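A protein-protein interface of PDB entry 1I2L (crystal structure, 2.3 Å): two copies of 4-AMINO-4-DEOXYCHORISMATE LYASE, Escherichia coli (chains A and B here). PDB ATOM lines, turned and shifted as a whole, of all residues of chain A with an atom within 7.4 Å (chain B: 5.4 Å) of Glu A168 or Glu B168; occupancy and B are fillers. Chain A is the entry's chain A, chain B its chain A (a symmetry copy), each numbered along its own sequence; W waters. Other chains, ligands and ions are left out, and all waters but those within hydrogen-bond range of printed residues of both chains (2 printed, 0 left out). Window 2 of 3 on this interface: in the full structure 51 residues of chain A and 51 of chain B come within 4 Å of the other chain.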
ATOM      1  N   ARG A 129     -35.109 -22.437 -16.622  1.00  0.00           N
ATOM      2  CA  ARG A 129     -34.378 -21.922 -17.764  1.00  0.00           C
ATOM      3  C   ARG A 129     -33.961 -23.058 -18.679  1.00  0.00           C
ATOM      4  O   ARG A 129     -33.533 -24.109 -18.220  1.00  0.00           O
ATOM      5  CB  ARG A 129     -33.160 -21.127 -17.300  1.00  0.00           C
ATOM      6  CG  ARG A 129     -33.531 -19.906 -16.494  1.00  0.00           C
ATOM      7  CD  ARG A 129     -32.338 -19.008 -16.247  1.00  0.00           C
ATOM      8  NE  ARG A 129     -32.746 -17.772 -15.595  1.00  0.00           N
ATOM      9  CZ  ARG A 129     -31.952 -16.726 -15.409  1.00  0.00           C
ATOM     10  NH1 ARG A 129     -30.696 -16.754 -15.829  1.00  0.00           N
ATOM     11  NH2 ARG A 129     -32.416 -15.651 -14.791  1.00  0.00           N
ATOM     12  N   LEU A 130     -34.105 -22.832 -19.978  1.00  0.00           N
ATOM     13  CA  LEU A 130     -33.758 -23.841 -20.967  1.00  0.00           C
ATOM     14  C   LEU A 130     -32.272 -24.083 -21.038  1.00  0.00           C
ATOM     15  O   LEU A 130     -31.476 -23.141 -21.071  1.00  0.00           O
ATOM     16  CB  LEU A 130     -34.246 -23.428 -22.365  1.00  0.00           C
ATOM     17  CG  LEU A 130     -35.738 -23.133 -22.550  1.00  0.00           C
ATOM     18  CD1 LEU A 130     -35.980 -22.680 -23.991  1.00  0.00           C
ATOM     19  CD2 LEU A 130     -36.555 -24.359 -22.217  1.00  0.00           C
ATOM     20  N   GLY A 131     -31.890 -25.350 -21.046  1.00  0.00           N
ATOM     21  CA  GLY A 131     -30.476 -25.644 -21.193  1.00  0.00           C
ATOM     22  C   GLY A 131     -30.137 -25.292 -22.631  1.00  0.00           C
ATOM     23  O   GLY A 131     -31.018 -25.304 -23.489  1.00  0.00           O
ATOM     24  N   ARG A 132     -28.882 -24.963 -22.909  1.00  0.00           N
ATOM     25  CA  ARG A 132     -28.486 -24.612 -24.271  1.00  0.00           C
ATOM     26  C   ARG A 132     -27.765 -25.793 -24.915  1.00  0.00           C
ATOM     27  O   ARG A 132     -26.918 -26.418 -24.286  1.00  0.00           O
ATOM     28  CB  ARG A 132     -27.604 -23.353 -24.248  1.00  0.00           C
ATOM     29  CG  ARG A 132     -28.366 -22.099 -23.784  1.00  0.00           C
ATOM     30  CD  ARG A 132     -27.438 -21.041 -23.189  1.00  0.00           C
ATOM     31  NE  ARG A 132     -26.345 -20.733 -24.100  1.00  0.00           N
ATOM     32  CZ  ARG A 132     -26.378 -19.781 -25.024  1.00  0.00           C
ATOM     33  NH1 ARG A 132     -27.456 -19.012 -25.161  1.00  0.00           N
ATOM     34  NH2 ARG A 132     -25.337 -19.624 -25.837  1.00  0.00           N
ATOM     35  N   LEU A 165     -36.402 -17.946 -20.417  1.00  0.00           N
ATOM     36  CA  LEU A 165     -35.027 -17.529 -20.655  1.00  0.00           C
ATOM     37  C   LEU A 165     -34.204 -18.794 -20.791  1.00  0.00           C
ATOM     38  O   LEU A 165     -34.677 -19.855 -20.414  1.00  0.00           O
ATOM     39  CB  LEU A 165     -34.501 -16.728 -19.462  1.00  0.00           C
ATOM     40  CG  LEU A 165     -35.338 -15.531 -19.022  1.00  0.00           C
ATOM     41  CD1 LEU A 165     -34.664 -14.844 -17.861  1.00  0.00           C
ATOM     42  CD2 LEU A 165     -35.486 -14.565 -20.173  1.00  0.00           C
ATOM     43  N   ASP A 166     -32.997 -18.710 -21.345  1.00  0.00           N
ATOM     44  CA  ASP A 166     -32.170 -19.904 -21.423  1.00  0.00           C
ATOM     45  C   ASP A 166     -31.202 -19.858 -20.234  1.00  0.00           C
ATOM     46  O   ASP A 166     -31.315 -18.947 -19.398  1.00  0.00           O
ATOM     47  CB  ASP A 166     -31.448 -20.032 -22.783  1.00  0.00           C
ATOM     48  CG  ASP A 166     -30.362 -18.985 -23.015  1.00  0.00           C
ATOM     49  OD1 ASP A 166     -29.934 -18.296 -22.071  1.00  0.00           O
ATOM     50  OD2 ASP A 166     -29.908 -18.868 -24.174  1.00  0.00           O
ATOM     51  N   SER A 167     -30.276 -20.819 -20.136  1.00  0.00           N
ATOM     52  CA  SER A 167     -29.325 -20.864 -19.015  1.00  0.00           C
ATOM     53  C   SER A 167     -28.353 -19.677 -18.933  1.00  0.00           C
ATOM     54  O   SER A 167     -27.692 -19.484 -17.915  1.00  0.00           O
ATOM     55  CB  SER A 167     -28.522 -22.179 -19.030  1.00  0.00           C
ATOM     56  OG  SER A 167     -27.726 -22.295 -20.193  1.00  0.00           O
ATOM     57  N   GLU A 168     -28.257 -18.888 -19.996  1.00  0.00           N
ATOM     58  CA  GLU A 168     -27.373 -17.735 -19.967  1.00  0.00           C
ATOM     59  C   GLU A 168     -28.154 -16.464 -19.655  1.00  0.00           C
ATOM     60  O   GLU A 168     -27.570 -15.397 -19.520  1.00  0.00           O
ATOM     61  CB  GLU A 168     -26.639 -17.587 -21.303  1.00  0.00           C
ATOM     62  CG  GLU A 168     -25.494 -18.580 -21.484  1.00  0.00           C
ATOM     63  CD  GLU A 168     -24.263 -18.204 -20.672  1.00  0.00           C
ATOM     64  OE1 GLU A 168     -23.590 -17.226 -21.063  1.00  0.00           O
ATOM     65  OE2 GLU A 168     -23.971 -18.871 -19.648  1.00  0.00           O
ATOM     66  N   GLY A 169     -29.473 -16.586 -19.534  1.00  0.00           N
ATOM     67  CA  GLY A 169     -30.312 -15.437 -19.248  1.00  0.00           C
ATOM     68  C   GLY A 169     -31.007 -14.837 -20.458  1.00  0.00           C
ATOM     69  O   GLY A 169     -31.781 -13.900 -20.313  1.00  0.00           O
ATOM     70  N   TRP A 170     -30.755 -15.370 -21.647  1.00  0.00           N
ATOM     71  CA  TRP A 170     -31.372 -14.851 -22.866  1.00  0.00           C
ATOM     72  C   TRP A 170     -32.841 -15.227 -23.058  1.00  0.00           C
ATOM     73  O   TRP A 170     -33.204 -16.403 -22.957  1.00  0.00           O
ATOM     74  CB  TRP A 170     -30.604 -15.337 -24.092  1.00  0.00           C
ATOM     75  CG  TRP A 170     -29.152 -15.059 -24.022  1.00  0.00           C
ATOM     76  CD1 TRP A 170     -28.146 -15.951 -24.192  1.00  0.00           C
ATOM     77  CD2 TRP A 170     -28.537 -13.799 -23.752  1.00  0.00           C
ATOM     78  NE1 TRP A 170     -26.931 -15.330 -24.041  1.00  0.00           N
ATOM     79  CE2 TRP A 170     -27.142 -14.005 -23.770  1.00  0.00           C
ATOM     80  CE3 TRP A 170     -29.029 -12.510 -23.499  1.00  0.00           C
ATOM     81  CZ2 TRP A 170     -26.227 -12.970 -23.542  1.00  0.00           C
ATOM     82  CZ3 TRP A 170     -28.126 -11.483 -23.272  1.00  0.00           C
ATOM     83  CH2 TRP A 170     -26.742 -11.718 -23.294  1.00  0.00           C
ATOM     84  N   VAL A 171     -33.680 -14.234 -23.360  1.00  0.00           N
ATOM     85  CA  VAL A 171     -35.090 -14.502 -23.594  1.00  0.00           C
ATOM     86  C   VAL A 171     -35.105 -15.436 -24.809  1.00  0.00           C
ATOM     87  O   VAL A 171     -34.471 -15.152 -25.818  1.00  0.00           O
ATOM     88  CB  VAL A 171     -35.875 -13.201 -23.914  1.00  0.00           C
ATOM     89  CG1 VAL A 171     -37.322 -13.532 -24.243  1.00  0.00           C
ATOM     90  CG2 VAL A 171     -35.822 -12.246 -22.731  1.00  0.00           C
ATOM     91  N   GLN A 194     -29.545 -21.835 -30.025  1.00  0.00           N
ATOM     92  CA  GLN A 194     -29.034 -22.428 -28.786  1.00  0.00           C
ATOM     93  C   GLN A 194     -30.100 -23.127 -27.933  1.00  0.00           C
ATOM     94  O   GLN A 194     -29.787 -24.007 -27.136  1.00  0.00           O
ATOM     95  CB  GLN A 194     -28.323 -21.353 -27.947  1.00  0.00           C
ATOM     96  CG  GLN A 194     -26.986 -20.931 -28.511  1.00  0.00           C
ATOM     97  CD  GLN A 194     -25.937 -22.045 -28.422  1.00  0.00           C
ATOM     98  OE1 GLN A 194     -25.018 -22.111 -29.239  1.00  0.00           O
ATOM     99  NE2 GLN A 194     -26.073 -22.918 -27.421  1.00  0.00           N
ATOM    100  N   GLN A 220     -30.194 -11.775 -29.312  1.00  0.00           N
ATOM    101  CA  GLN A 220     -29.850 -12.440 -28.070  1.00  0.00           C
ATOM    102  C   GLN A 220     -30.153 -11.301 -27.113  1.00  0.00           C
ATOM    103  O   GLN A 220     -29.364 -10.356 -27.005  1.00  0.00           O
ATOM    104  CB  GLN A 220     -28.369 -12.760 -27.987  1.00  0.00           C
ATOM    105  CG  GLN A 220     -28.000 -14.088 -28.568  1.00  0.00           C
ATOM    106  CD  GLN A 220     -26.691 -14.572 -28.018  1.00  0.00           C
ATOM    107  OE1 GLN A 220     -26.269 -15.694 -28.285  1.00  0.00           O
ATOM    108  NE2 GLN A 220     -26.034 -13.720 -27.232  1.00  0.00           N
ATOM    109  N   SER A 222     -31.619  -9.833 -23.183  1.00  0.00           N
ATOM    110  CA  SER A 222     -31.851 -10.049 -21.759  1.00  0.00           C
ATOM    111  C   SER A 222     -33.304  -9.757 -21.490  1.00  0.00           C
ATOM    112  O   SER A 222     -33.978  -9.142 -22.318  1.00  0.00           O
ATOM    113  CB  SER A 222     -31.016  -9.085 -20.932  1.00  0.00           C
ATOM    114  OG  SER A 222     -31.428  -7.753 -21.194  1.00  0.00           O
ATOM    115  N   ARG B 129     -22.485 -31.166 -26.293  1.00  0.00           N
ATOM    116  CA  ARG B 129     -22.378 -30.734 -24.913  1.00  0.00           C
ATOM    117  C   ARG B 129     -23.752 -30.679 -24.270  1.00  0.00           C
ATOM    118  O   ARG B 129     -24.713 -30.232 -24.881  1.00  0.00           O
ATOM    119  CB  ARG B 129     -21.690 -29.374 -24.834  1.00  0.00           C
ATOM    120  CG  ARG B 129     -20.269 -29.407 -25.340  1.00  0.00           C
ATOM    121  CD  ARG B 129     -19.531 -28.122 -25.037  1.00  0.00           C
ATOM    122  NE  ARG B 129     -18.126 -28.232 -25.406  1.00  0.00           N
ATOM    123  CZ  ARG B 129     -17.199 -27.332 -25.102  1.00  0.00           C
ATOM    124  NH1 ARG B 129     -17.519 -26.245 -24.415  1.00  0.00           N
ATOM    125  NH2 ARG B 129     -15.949 -27.518 -25.496  1.00  0.00           N
ATOM    126  N   ARG B 132     -27.372 -27.125 -19.625  1.00  0.00           N
ATOM    127  CA  ARG B 132     -27.425 -27.089 -18.166  1.00  0.00           C
ATOM    128  C   ARG B 132     -28.822 -26.672 -17.714  1.00  0.00           C
ATOM    129  O   ARG B 132     -29.399 -25.740 -18.266  1.00  0.00           O
ATOM    130  CB  ARG B 132     -26.347 -26.132 -17.631  1.00  0.00           C
ATOM    131  CG  ARG B 132     -24.917 -26.631 -17.904  1.00  0.00           C
ATOM    132  CD  ARG B 132     -23.901 -25.490 -17.945  1.00  0.00           C
ATOM    133  NE  ARG B 132     -23.992 -24.666 -16.748  1.00  0.00           N
ATOM    134  CZ  ARG B 132     -23.298 -24.870 -15.636  1.00  0.00           C
ATOM    135  NH1 ARG B 132     -22.430 -25.877 -15.559  1.00  0.00           N
ATOM    136  NH2 ARG B 132     -23.503 -24.082 -14.585  1.00  0.00           N
ATOM    137  N   ASP B 166     -20.375 -30.121 -20.368  1.00  0.00           N
ATOM    138  CA  ASP B 166     -21.664 -29.449 -20.422  1.00  0.00           C
ATOM    139  C   ASP B 166     -21.481 -28.193 -21.283  1.00  0.00           C
ATOM    140  O   ASP B 166     -20.388 -27.996 -21.839  1.00  0.00           O
ATOM    141  CB  ASP B 166     -22.225 -29.139 -19.016  1.00  0.00           C
ATOM    142  CG  ASP B 166     -21.443 -28.073 -18.251  1.00  0.00           C
ATOM    143  OD1 ASP B 166     -20.620 -27.348 -18.840  1.00  0.00           O
ATOM    144  OD2 ASP B 166     -21.680 -27.945 -17.031  1.00  0.00           O
ATOM    145  N   SER B 167     -22.519 -27.358 -21.413  1.00  0.00           N
ATOM    146  CA  SER B 167     -22.436 -26.145 -22.239  1.00  0.00           C
ATOM    147  C   SER B 167     -21.427 -25.091 -21.757  1.00  0.00           C
ATOM    148  O   SER B 167     -21.097 -24.164 -22.493  1.00  0.00           O
ATOM    149  CB  SER B 167     -23.822 -25.489 -22.390  1.00  0.00           C
ATOM    150  OG  SER B 167     -24.335 -25.053 -21.147  1.00  0.00           O
ATOM    151  N   GLU B 168     -20.942 -25.224 -20.528  1.00  0.00           N
ATOM    152  CA  GLU B 168     -19.964 -24.273 -20.026  1.00  0.00           C
ATOM    153  C   GLU B 168     -18.552 -24.830 -20.159  1.00  0.00           C
ATOM    154  O   GLU B 168     -17.586 -24.144 -19.853  1.00  0.00           O
ATOM    155  CB  GLU B 168     -20.257 -23.921 -18.565  1.00  0.00           C
ATOM    156  CG  GLU B 168     -21.427 -22.957 -18.392  1.00  0.00           C
ATOM    157  CD  GLU B 168     -21.058 -21.524 -18.747  1.00  0.00           C
ATOM    158  OE1 GLU B 168     -20.317 -20.904 -17.954  1.00  0.00           O
ATOM    159  OE2 GLU B 168     -21.495 -21.020 -19.813  1.00  0.00           O
ATOM    160  N   GLY B 169     -18.439 -26.071 -20.624  1.00  0.00           N
ATOM    161  CA  GLY B 169     -17.141 -26.701 -20.779  1.00  0.00           C
ATOM    162  C   GLY B 169     -16.752 -27.648 -19.656  1.00  0.00           C
ATOM    163  O   GLY B 169     -15.702 -28.272 -19.723  1.00  0.00           O
ATOM    164  N   TRP B 170     -17.589 -27.775 -18.634  1.00  0.00           N
ATOM    165  CA  TRP B 170     -17.292 -28.656 -17.506  1.00  0.00           C
ATOM    166  C   TRP B 170     -17.475 -30.148 -17.784  1.00  0.00           C
ATOM    167  O   TRP B 170     -18.522 -30.566 -18.288  1.00  0.00           O
ATOM    168  CB  TRP B 170     -18.171 -28.295 -16.312  1.00  0.00           C
ATOM    169  CG  TRP B 170     -18.108 -26.861 -15.950  1.00  0.00           C
ATOM    170  CD1 TRP B 170     -19.158 -26.018 -15.792  1.00  0.00           C
ATOM    171  CD2 TRP B 170     -16.929 -26.093 -15.709  1.00  0.00           C
ATOM    172  NE1 TRP B 170     -18.711 -24.760 -15.470  1.00  0.00           N
ATOM    173  CE2 TRP B 170     -17.343 -24.778 -15.412  1.00  0.00           C
ATOM    174  CE3 TRP B 170     -15.558 -26.388 -15.712  1.00  0.00           C
ATOM    175  CZ2 TRP B 170     -16.436 -23.753 -15.120  1.00  0.00           C
ATOM    176  CZ3 TRP B 170     -14.656 -25.375 -15.424  1.00  0.00           C
ATOM    177  CH2 TRP B 170     -15.098 -24.074 -15.134  1.00  0.00           C
HETATM  178  O   HOH W   1     -31.176 -23.957 -17.340  1.00  0.00           O
HETATM  179  O   HOH W   2     -24.714 -27.720 -25.091  1.00  0.00           O
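The side-chain carboxylate (OE2) of Glu A168 sits close to the side-chain carboxylate (OE2) of Glu B168 (3.3 Å).
The side-chain carboxylate of Asp A166 is in hydrogen-bond range of the backbone NH of Glu A168 (2.7 Å).
The guanidinium group of Arg A132 lies within salt-bridge range of the side-chain carboxylate of Asp A166, at 2.6 Å.
The side-chain carboxylate (OD2) of Asp B166 lies within salt-bridge range of the guanidinium group (NH1) of Arg B132 (2.6 Å).
The backbone NH of Ser A167 lies within hydrogen-bond range of the backbone carbonyl oxygen of Leu A130 (2.8 Å).
OD1 of Asp B166 lies within hydrogen-bond range of N of Glu B168 (2.7 Å).
Among the printed residues, pairs that only touch across the chains: Gly A131 with Arg B132 (3.1 Å), Arg A132 with Ser B167 (3.7 Å) and Ser A167 with Arg B132 (3.7 Å).
Of the printed residues of chain B, Glu A168 touches Glu B168 (3.3 Å).
Glu B168 touches one residue of chain A.
Printed residues of chain A within 4 Å of Ser B167: Arg A132.
Of the printed residues of chain A, Arg B132 touches Gly A131 and Ser A167.
Leu A130 touches none of the printed residues of chain B.
The nearest printed residue of chain B that does not touch Glu A168 is Ser B167 (6.4 Å).
The nearest residue of chain A that does not touch Glu B168 is Ser A167 (6.4 Å).
The nearest printed residue of chain B that does not touch Gly A131 is Ser B167 (6.0 Å).
Among the printed residues, no Asp or Glu carboxylate lies within 4 Å of a Lys or Arg side-chain nitrogen of the other chain.
Arg A132 touches Ser B167, and with the chains exchanged Ser A167 touches Arg B132.
Glu B168 touches its own counterpart, Glu A168.
Positions printed for both chains: 129, 132, 166, 167, 168, 169 and 170.
Water W2 lies within hydrogen-bond range of O of Arg B129 (2.5 Å) and O of Arg A132 (2.7 Å).
Water W1 lies within hydrogen-bond range of the backbone carbonyl oxygen of Arg A129 (2.5 Å) and the backbone carbonyl oxygen of Arg B132 (2.7 Å).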
